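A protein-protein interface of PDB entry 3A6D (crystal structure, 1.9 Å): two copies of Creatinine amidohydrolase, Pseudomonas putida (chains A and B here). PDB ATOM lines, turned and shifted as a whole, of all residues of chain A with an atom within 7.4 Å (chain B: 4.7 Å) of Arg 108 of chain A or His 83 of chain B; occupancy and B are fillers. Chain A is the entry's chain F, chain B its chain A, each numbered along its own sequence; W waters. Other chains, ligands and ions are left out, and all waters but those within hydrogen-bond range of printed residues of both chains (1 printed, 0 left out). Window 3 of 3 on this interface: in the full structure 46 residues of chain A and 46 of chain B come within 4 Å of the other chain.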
ATOM      1  N   TRP A  12     -30.106  -8.227  -6.494  1.00  0.00           N
ATOM      2  CA  TRP A  12     -30.352  -6.865  -6.940  1.00  0.00           C
ATOM      3  C   TRP A  12     -31.499  -6.819  -7.944  1.00  0.00           C
ATOM      4  O   TRP A  12     -32.177  -5.804  -8.069  1.00  0.00           O
ATOM      5  CB  TRP A  12     -29.092  -6.230  -7.540  1.00  0.00           C
ATOM      6  CG  TRP A  12     -28.648  -6.752  -8.876  1.00  0.00           C
ATOM      7  CD1 TRP A  12     -27.757  -7.762  -9.111  1.00  0.00           C
ATOM      8  CD2 TRP A  12     -28.998  -6.220 -10.162  1.00  0.00           C
ATOM      9  NE1 TRP A  12     -27.520  -7.882 -10.461  1.00  0.00           N
ATOM     10  CE2 TRP A  12     -28.271  -6.950 -11.129  1.00  0.00           C
ATOM     11  CE3 TRP A  12     -29.855  -5.195 -10.587  1.00  0.00           C
ATOM     12  CZ2 TRP A  12     -28.370  -6.684 -12.500  1.00  0.00           C
ATOM     13  CZ3 TRP A  12     -29.956  -4.930 -11.948  1.00  0.00           C
ATOM     14  CH2 TRP A  12     -29.215  -5.674 -12.889  1.00  0.00           C
ATOM     15  N   ILE A 102     -27.312   6.751   3.292  1.00  0.00           N
ATOM     16  CA  ILE A 102     -28.276   5.719   2.933  1.00  0.00           C
ATOM     17  C   ILE A 102     -29.468   6.296   2.168  1.00  0.00           C
ATOM     18  O   ILE A 102     -29.914   5.714   1.180  1.00  0.00           O
ATOM     19  CB  ILE A 102     -28.743   4.943   4.193  1.00  0.00           C
ATOM     20  CG1 ILE A 102     -27.590   4.064   4.695  1.00  0.00           C
ATOM     21  CG2 ILE A 102     -29.964   4.086   3.882  1.00  0.00           C
ATOM     22  CD1 ILE A 102     -27.826   3.459   6.067  1.00  0.00           C
ATOM     23  N   ILE A 103     -29.980   7.438   2.609  1.00  0.00           N
ATOM     24  CA  ILE A 103     -31.102   8.052   1.911  1.00  0.00           C
ATOM     25  C   ILE A 103     -30.696   8.457   0.488  1.00  0.00           C
ATOM     26  O   ILE A 103     -31.468   8.286  -0.447  1.00  0.00           O
ATOM     27  CB  ILE A 103     -31.646   9.270   2.695  1.00  0.00           C
ATOM     28  CG1 ILE A 103     -32.263   8.782   4.012  1.00  0.00           C
ATOM     29  CG2 ILE A 103     -32.687  10.019   1.857  1.00  0.00           C
ATOM     30  CD1 ILE A 103     -32.692   9.892   4.971  1.00  0.00           C
ATOM     31  N   ARG A 104     -29.483   8.982   0.320  1.00  0.00           N
ATOM     32  CA  ARG A 104     -28.997   9.367  -1.009  1.00  0.00           C
ATOM     33  C   ARG A 104     -29.014   8.163  -1.960  1.00  0.00           C
ATOM     34  O   ARG A 104     -29.461   8.261  -3.111  1.00  0.00           O
ATOM     35  CB  ARG A 104     -27.562   9.910  -0.917  1.00  0.00           C
ATOM     36  CG  ARG A 104     -26.880  10.157  -2.265  1.00  0.00           C
ATOM     37  CD  ARG A 104     -25.403  10.543  -2.085  1.00  0.00           C
ATOM     38  NE  ARG A 104     -25.265  11.661  -1.157  1.00  0.00           N
ATOM     39  CZ  ARG A 104     -24.591  11.612  -0.010  1.00  0.00           C
ATOM     40  NH1 ARG A 104     -24.538  12.688   0.765  1.00  0.00           N
ATOM     41  NH2 ARG A 104     -23.957  10.501   0.356  1.00  0.00           N
ATOM     42  N   GLU A 105     -28.527   7.029  -1.470  1.00  0.00           N
ATOM     43  CA  GLU A 105     -28.463   5.818  -2.272  1.00  0.00           C
ATOM     44  C   GLU A 105     -29.847   5.256  -2.606  1.00  0.00           C
ATOM     45  O   GLU A 105     -30.114   4.892  -3.752  1.00  0.00           O
ATOM     46  CB  GLU A 105     -27.607   4.775  -1.550  1.00  0.00           C
ATOM     47  CG  GLU A 105     -26.127   5.147  -1.557  1.00  0.00           C
ATOM     48  CD  GLU A 105     -25.482   4.911  -2.909  1.00  0.00           C
ATOM     49  OE1 GLU A 105     -24.949   3.797  -3.121  1.00  0.00           O
ATOM     50  OE2 GLU A 105     -25.517   5.824  -3.768  1.00  0.00           O
ATOM     51  N   LEU A 106     -30.726   5.192  -1.613  1.00  0.00           N
ATOM     52  CA  LEU A 106     -32.076   4.684  -1.848  1.00  0.00           C
ATOM     53  C   LEU A 106     -32.780   5.549  -2.894  1.00  0.00           C
ATOM     54  O   LEU A 106     -33.504   5.035  -3.756  1.00  0.00           O
ATOM     55  CB  LEU A 106     -32.877   4.668  -0.544  1.00  0.00           C
ATOM     56  CG  LEU A 106     -32.406   3.663   0.517  1.00  0.00           C
ATOM     57  CD1 LEU A 106     -33.319   3.748   1.731  1.00  0.00           C
ATOM     58  CD2 LEU A 106     -32.411   2.250  -0.057  1.00  0.00           C
ATOM     59  N   ALA A 107     -32.562   6.861  -2.828  1.00  0.00           N
ATOM     60  CA  ALA A 107     -33.173   7.770  -3.794  1.00  0.00           C
ATOM     61  C   ALA A 107     -32.609   7.466  -5.179  1.00  0.00           C
ATOM     62  O   ALA A 107     -33.340   7.474  -6.176  1.00  0.00           O
ATOM     63  CB  ALA A 107     -32.888   9.218  -3.415  1.00  0.00           C
ATOM     64  N   ARG A 108     -31.309   7.190  -5.244  1.00  0.00           N
ATOM     65  CA  ARG A 108     -30.687   6.864  -6.520  1.00  0.00           C
ATOM     66  C   ARG A 108     -31.330   5.601  -7.099  1.00  0.00           C
ATOM     67  O   ARG A 108     -31.490   5.489  -8.314  1.00  0.00           O
ATOM     68  CB  ARG A 108     -29.177   6.647  -6.359  1.00  0.00           C
ATOM     69  CG  ARG A 108     -28.497   6.117  -7.625  1.00  0.00           C
ATOM     70  CD  ARG A 108     -26.990   5.971  -7.437  1.00  0.00           C
ATOM     71  NE  ARG A 108     -26.640   5.021  -6.383  1.00  0.00           N
ATOM     72  CZ  ARG A 108     -26.784   3.701  -6.475  1.00  0.00           C
ATOM     73  NH1 ARG A 108     -27.277   3.154  -7.578  1.00  0.00           N
ATOM     74  NH2 ARG A 108     -26.423   2.923  -5.463  1.00  0.00           N
ATOM     75  N   HIS A 109     -31.700   4.660  -6.229  1.00  0.00           N
ATOM     76  CA  HIS A 109     -32.339   3.411  -6.660  1.00  0.00           C
ATOM     77  C   HIS A 109     -33.717   3.694  -7.256  1.00  0.00           C
ATOM     78  O   HIS A 109     -34.229   2.914  -8.062  1.00  0.00           O
ATOM     79  CB  HIS A 109     -32.537   2.454  -5.476  1.00  0.00           C
ATOM     80  CG  HIS A 109     -31.268   2.029  -4.805  1.00  0.00           C
ATOM     81  ND1 HIS A 109     -31.253   1.437  -3.561  1.00  0.00           N
ATOM     82  CD2 HIS A 109     -29.974   2.107  -5.200  1.00  0.00           C
ATOM     83  CE1 HIS A 109     -30.007   1.172  -3.215  1.00  0.00           C
ATOM     84  NE2 HIS A 109     -29.210   1.568  -4.192  1.00  0.00           N
ATOM     85  N   GLY A 110     -34.322   4.801  -6.836  1.00  0.00           N
ATOM     86  CA  GLY A 110     -35.643   5.153  -7.323  1.00  0.00           C
ATOM     87  C   GLY A 110     -36.670   5.056  -6.211  1.00  0.00           C
ATOM     88  O   GLY A 110     -37.850   5.342  -6.418  1.00  0.00           O
ATOM     89  N   ALA A 111     -36.225   4.643  -5.027  1.00  0.00           N
ATOM     90  CA  ALA A 111     -37.121   4.526  -3.885  1.00  0.00           C
ATOM     91  C   ALA A 111     -37.540   5.932  -3.463  1.00  0.00           C
ATOM     92  O   ALA A 111     -36.771   6.884  -3.620  1.00  0.00           O
ATOM     93  CB  ALA A 111     -36.415   3.816  -2.731  1.00  0.00           C
ATOM     94  N   ARG A 112     -38.751   6.058  -2.932  1.00  0.00           N
ATOM     95  CA  ARG A 112     -39.267   7.354  -2.500  1.00  0.00           C
ATOM     96  C   ARG A 112     -40.057   7.283  -1.194  1.00  0.00           C
ATOM     97  O   ARG A 112     -40.656   8.271  -0.766  1.00  0.00           O
ATOM     98  CB  ARG A 112     -40.153   7.949  -3.599  1.00  0.00           C
ATOM     99  CG  ARG A 112     -39.384   8.387  -4.838  1.00  0.00           C
ATOM    100  CD  ARG A 112     -38.513   9.604  -4.530  1.00  0.00           C
ATOM    101  NE  ARG A 112     -37.873  10.169  -5.717  1.00  0.00           N
ATOM    102  CZ  ARG A 112     -36.762   9.698  -6.274  1.00  0.00           C
ATOM    103  NH1 ARG A 112     -36.144   8.637  -5.758  1.00  0.00           N
ATOM    104  NH2 ARG A 112     -36.257  10.298  -7.345  1.00  0.00           N
ATOM    105  N   LEU A 138     -31.439  16.249  -2.176  1.00  0.00           N
ATOM    106  CA  LEU A 138     -32.389  15.791  -3.183  1.00  0.00           C
ATOM    107  C   LEU A 138     -33.044  17.014  -3.817  1.00  0.00           C
ATOM    108  O   LEU A 138     -33.340  17.027  -5.012  1.00  0.00           O
ATOM    109  CB  LEU A 138     -33.447  14.876  -2.552  1.00  0.00           C
ATOM    110  CG  LEU A 138     -32.963  13.462  -2.212  1.00  0.00           C
ATOM    111  CD1 LEU A 138     -34.081  12.665  -1.543  1.00  0.00           C
ATOM    112  CD2 LEU A 138     -32.503  12.776  -3.495  1.00  0.00           C
ATOM    113  N   ILE A 143     -35.623  17.114  -6.751  1.00  0.00           N
ATOM    114  CA  ILE A 143     -36.403  15.997  -6.239  1.00  0.00           C
ATOM    115  C   ILE A 143     -37.049  16.363  -4.905  1.00  0.00           C
ATOM    116  O   ILE A 143     -36.358  16.682  -3.935  1.00  0.00           O
ATOM    117  CB  ILE A 143     -35.510  14.751  -6.048  1.00  0.00           C
ATOM    118  CG1 ILE A 143     -34.915  14.332  -7.392  1.00  0.00           C
ATOM    119  CG2 ILE A 143     -36.320  13.610  -5.440  1.00  0.00           C
ATOM    120  CD1 ILE A 143     -33.851  13.254  -7.287  1.00  0.00           C
ATOM    121  N   PHE A 146     -39.529  12.457  -2.239  1.00  0.00           N
ATOM    122  CA  PHE A 146     -39.017  11.408  -1.355  1.00  0.00           C
ATOM    123  C   PHE A 146     -39.604  11.724   0.019  1.00  0.00           C
ATOM    124  O   PHE A 146     -39.425  12.831   0.538  1.00  0.00           O
ATOM    125  CB  PHE A 146     -37.482  11.427  -1.301  1.00  0.00           C
ATOM    126  CG  PHE A 146     -36.882  10.205  -0.654  1.00  0.00           C
ATOM    127  CD1 PHE A 146     -37.030   9.978   0.710  1.00  0.00           C
ATOM    128  CD2 PHE A 146     -36.184   9.273  -1.416  1.00  0.00           C
ATOM    129  CE1 PHE A 146     -36.491   8.838   1.308  1.00  0.00           C
ATOM    130  CE2 PHE A 146     -35.643   8.131  -0.829  1.00  0.00           C
ATOM    131  CZ  PHE A 146     -35.796   7.914   0.535  1.00  0.00           C
ATOM    132  N   GLY B  80     -18.239  -4.208  -9.805  1.00  0.00           N
ATOM    133  CA  GLY B  80     -19.282  -3.944 -10.783  1.00  0.00           C
ATOM    134  C   GLY B  80     -19.613  -2.477 -10.995  1.00  0.00           C
ATOM    135  O   GLY B  80     -19.871  -2.055 -12.125  1.00  0.00           O
ATOM    136  N   GLY B  81     -19.616  -1.693  -9.919  1.00  0.00           N
ATOM    137  CA  GLY B  81     -19.923  -0.278 -10.048  1.00  0.00           C
ATOM    138  C   GLY B  81     -21.055   0.147  -9.132  1.00  0.00           C
ATOM    139  O   GLY B  81     -21.946  -0.643  -8.829  1.00  0.00           O
ATOM    140  N   ASN B  82     -21.038   1.405  -8.702  1.00  0.00           N
ATOM    141  CA  ASN B  82     -22.062   1.895  -7.791  1.00  0.00           C
ATOM    142  C   ASN B  82     -23.347   2.355  -8.473  1.00  0.00           C
ATOM    143  O   ASN B  82     -24.204   2.966  -7.830  1.00  0.00           O
ATOM    144  CB  ASN B  82     -21.496   3.035  -6.940  1.00  0.00           C
ATOM    145  CG  ASN B  82     -22.138   3.104  -5.574  1.00  0.00           C
ATOM    146  OD1 ASN B  82     -22.937   3.997  -5.287  1.00  0.00           O
ATOM    147  ND2 ASN B  82     -21.806   2.143  -4.725  1.00  0.00           N
ATOM    148  N   HIS B  83     -23.480   2.063  -9.764  1.00  0.00           N
ATOM    149  CA  HIS B  83     -24.672   2.451 -10.514  1.00  0.00           C
ATOM    150  C   HIS B  83     -25.790   1.413 -10.406  1.00  0.00           C
ATOM    151  O   HIS B  83     -26.932   1.680 -10.788  1.00  0.00           O
ATOM    152  CB  HIS B  83     -24.323   2.670 -11.991  1.00  0.00           C
ATOM    153  CG  HIS B  83     -23.751   1.461 -12.663  1.00  0.00           C
ATOM    154  ND1 HIS B  83     -22.515   0.943 -12.337  1.00  0.00           N
ATOM    155  CD2 HIS B  83     -24.245   0.664 -13.641  1.00  0.00           C
ATOM    156  CE1 HIS B  83     -22.273  -0.118 -13.086  1.00  0.00           C
ATOM    157  NE2 HIS B  83     -23.306  -0.308 -13.886  1.00  0.00           N
ATOM    158  N   PHE B  84     -25.469   0.230  -9.890  1.00  0.00           N
ATOM    159  CA  PHE B  84     -26.468  -0.824  -9.742  1.00  0.00           C
ATOM    160  C   PHE B  84     -27.465  -0.550  -8.623  1.00  0.00           C
ATOM    161  O   PHE B  84     -27.141   0.114  -7.637  1.00  0.00           O
ATOM    162  CB  PHE B  84     -25.810  -2.172  -9.428  1.00  0.00           C
ATOM    163  CG  PHE B  84     -25.207  -2.857 -10.617  1.00  0.00           C
ATOM    164  CD1 PHE B  84     -23.944  -2.501 -11.078  1.00  0.00           C
ATOM    165  CD2 PHE B  84     -25.900  -3.876 -11.268  1.00  0.00           C
ATOM    166  CE1 PHE B  84     -23.375  -3.153 -12.169  1.00  0.00           C
ATOM    167  CE2 PHE B  84     -25.343  -4.535 -12.362  1.00  0.00           C
ATOM    168  CZ  PHE B  84     -24.078  -4.174 -12.813  1.00  0.00           C
ATOM    169  N   PRO B  85     -28.701  -1.060  -8.770  1.00  0.00           N
ATOM    170  CA  PRO B  85     -29.751  -0.892  -7.763  1.00  0.00           C
ATOM    171  C   PRO B  85     -29.339  -1.789  -6.602  1.00  0.00           C
ATOM    172  O   PRO B  85     -28.535  -2.702  -6.789  1.00  0.00           O
ATOM    173  CB  PRO B  85     -30.997  -1.446  -8.458  1.00  0.00           C
ATOM    174  CG  PRO B  85     -30.698  -1.284  -9.920  1.00  0.00           C
ATOM    175  CD  PRO B  85     -29.246  -1.673  -9.995  1.00  0.00           C
ATOM    176  N   THR B  87     -27.196  -1.793  -4.297  1.00  0.00           N
ATOM    177  CA  THR B  87     -25.939  -1.357  -3.701  1.00  0.00           C
ATOM    178  C   THR B  87     -26.210  -0.037  -2.973  1.00  0.00           C
ATOM    179  O   THR B  87     -26.694   0.926  -3.574  1.00  0.00           O
ATOM    180  CB  THR B  87     -24.861  -1.147  -4.784  1.00  0.00           C
ATOM    181  OG1 THR B  87     -24.658  -2.377  -5.496  1.00  0.00           O
ATOM    182  CG2 THR B  87     -23.536  -0.706  -4.148  1.00  0.00           C
ATOM    183  N   VAL B 216     -19.098   6.228 -14.140  1.00  0.00           N
ATOM    184  CA  VAL B 216     -18.978   4.819 -14.482  1.00  0.00           C
ATOM    185  C   VAL B 216     -19.867   4.462 -15.670  1.00  0.00           C
ATOM    186  O   VAL B 216     -21.049   4.810 -15.713  1.00  0.00           O
ATOM    187  CB  VAL B 216     -19.330   3.918 -13.276  1.00  0.00           C
ATOM    188  CG1 VAL B 216     -20.752   4.194 -12.807  1.00  0.00           C
ATOM    189  CG2 VAL B 216     -19.156   2.452 -13.656  1.00  0.00           C
ATOM    190  N   PRO B 218     -21.827   1.798 -17.462  1.00  0.00           N
ATOM    191  CA  PRO B 218     -22.512   0.518 -17.247  1.00  0.00           C
ATOM    192  C   PRO B 218     -22.167  -0.560 -18.271  1.00  0.00           C
ATOM    193  O   PRO B 218     -22.124  -1.748 -17.950  1.00  0.00           O
ATOM    194  CB  PRO B 218     -23.988   0.902 -17.311  1.00  0.00           C
ATOM    195  CG  PRO B 218     -23.989   2.308 -16.801  1.00  0.00           C
ATOM    196  CD  PRO B 218     -22.802   2.903 -17.510  1.00  0.00           C
ATOM    197  N   THR B 221     -19.274  -3.179 -17.592  1.00  0.00           N
ATOM    198  CA  THR B 221     -19.424  -4.194 -16.551  1.00  0.00           C
ATOM    199  C   THR B 221     -20.328  -5.288 -17.111  1.00  0.00           C
ATOM    200  O   THR B 221     -21.291  -4.990 -17.810  1.00  0.00           O
ATOM    201  CB  THR B 221     -20.117  -3.631 -15.280  1.00  0.00           C
ATOM    202  OG1 THR B 221     -19.288  -2.636 -14.667  1.00  0.00           O
ATOM    203  CG2 THR B 221     -20.383  -4.744 -14.281  1.00  0.00           C
HETATM  204  O   HOH W   1     -27.879   4.121 -10.206  1.00  0.00           O
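OD1 of Asn 82 of chain B sits close to OE1 of Glu 105 of chain A.
The guanidinium group of Arg 108 of chain A sits close to the backbone carbonyl oxygen of Asn 82 of chain B (3.1 Å).
The backbone carbonyl oxygen of Phe 84 of chain B lies within hydrogen-bond range of the guanidinium group of Arg 108 of chain A (3.0 Å).
The backbone carbonyl oxygen (O) of Thr 87 of chain B lies within hydrogen-bond range of a ring nitrogen (NE2) of His 109 of chain A (2.7 Å).
The side-chain carboxylate (OE1) of Glu 105 of chain A lies close to the backbone carbonyl oxygen (O) of Thr 87 of chain B (3.4 Å).
O of Thr 87 of chain B is in hydrogen-bond range of NH2 of Arg 108 of chain A.
The backbone carbonyl oxygen (O) of Glu 105 of chain A lies close to a ring nitrogen (NE2) of His 109 of chain A, 3.5 Å away.
The side-chain carboxylate (OE1) of Glu 105 of chain A lies within salt-bridge range of the guanidinium group (NH2) of Arg 108 of chain A (2.9 Å).
NH2 of Arg 108 of chain A lies within hydrogen-bond range of NE2 of His 109 of chain A, at 3.3 Å.
Among the printed residues, pairs that only touch across the chains: Trp 12 of chain A with Phe 84 of chain B (3.7 Å), Trp 12 of chain A with Pro 85 of chain B (3.6 Å), Arg 108 of chain A with His 83 of chain B (3.5 Å) and His 109 of chain A with Pro 85 of chain B (3.95 Å).
Of chain B, only Asn 82 (3.0 Å), His 83 (3.5 Å), Phe 84 (3.0 Å) and Thr 87 (2.8 Å) come within 4 Å of Arg 108 of chain A.
Of chain A, only Arg 108 comes within 4 Å of His 83 of chain B.
Of the printed residues of chain A, Thr 87 of chain B touches Glu 105, Arg 108 and His 109.
Printed residues of chain A within 4 Å of Pro 85 of chain B: Trp 12 (3.6 Å) and His 109 (3.95 Å).
The nearest residue of chain B that does not touch Arg 108 of chain A is Pro 85 of chain B (4.6 Å).
The nearest residue of chain A that does not touch His 83 of chain B is His 109 of chain A (6.4 Å).
Hydrophobic or aromatic side chains of chain B that line the printed part of chain A: Phe 84 and Pro 85.
Printed residues of chain A that touch a printed residue of chain B: Trp 12, Glu 105, Arg 108 and His 109.
Among the printed residues, no Asp or Glu carboxylate lies within 4 Å of a Lys or Arg side-chain nitrogen of the other chain.
No position is printed for both chains.
Water W1 lies within hydrogen-bond range of O of His 83 of chain B and NH1 of Arg 108 of chain A.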
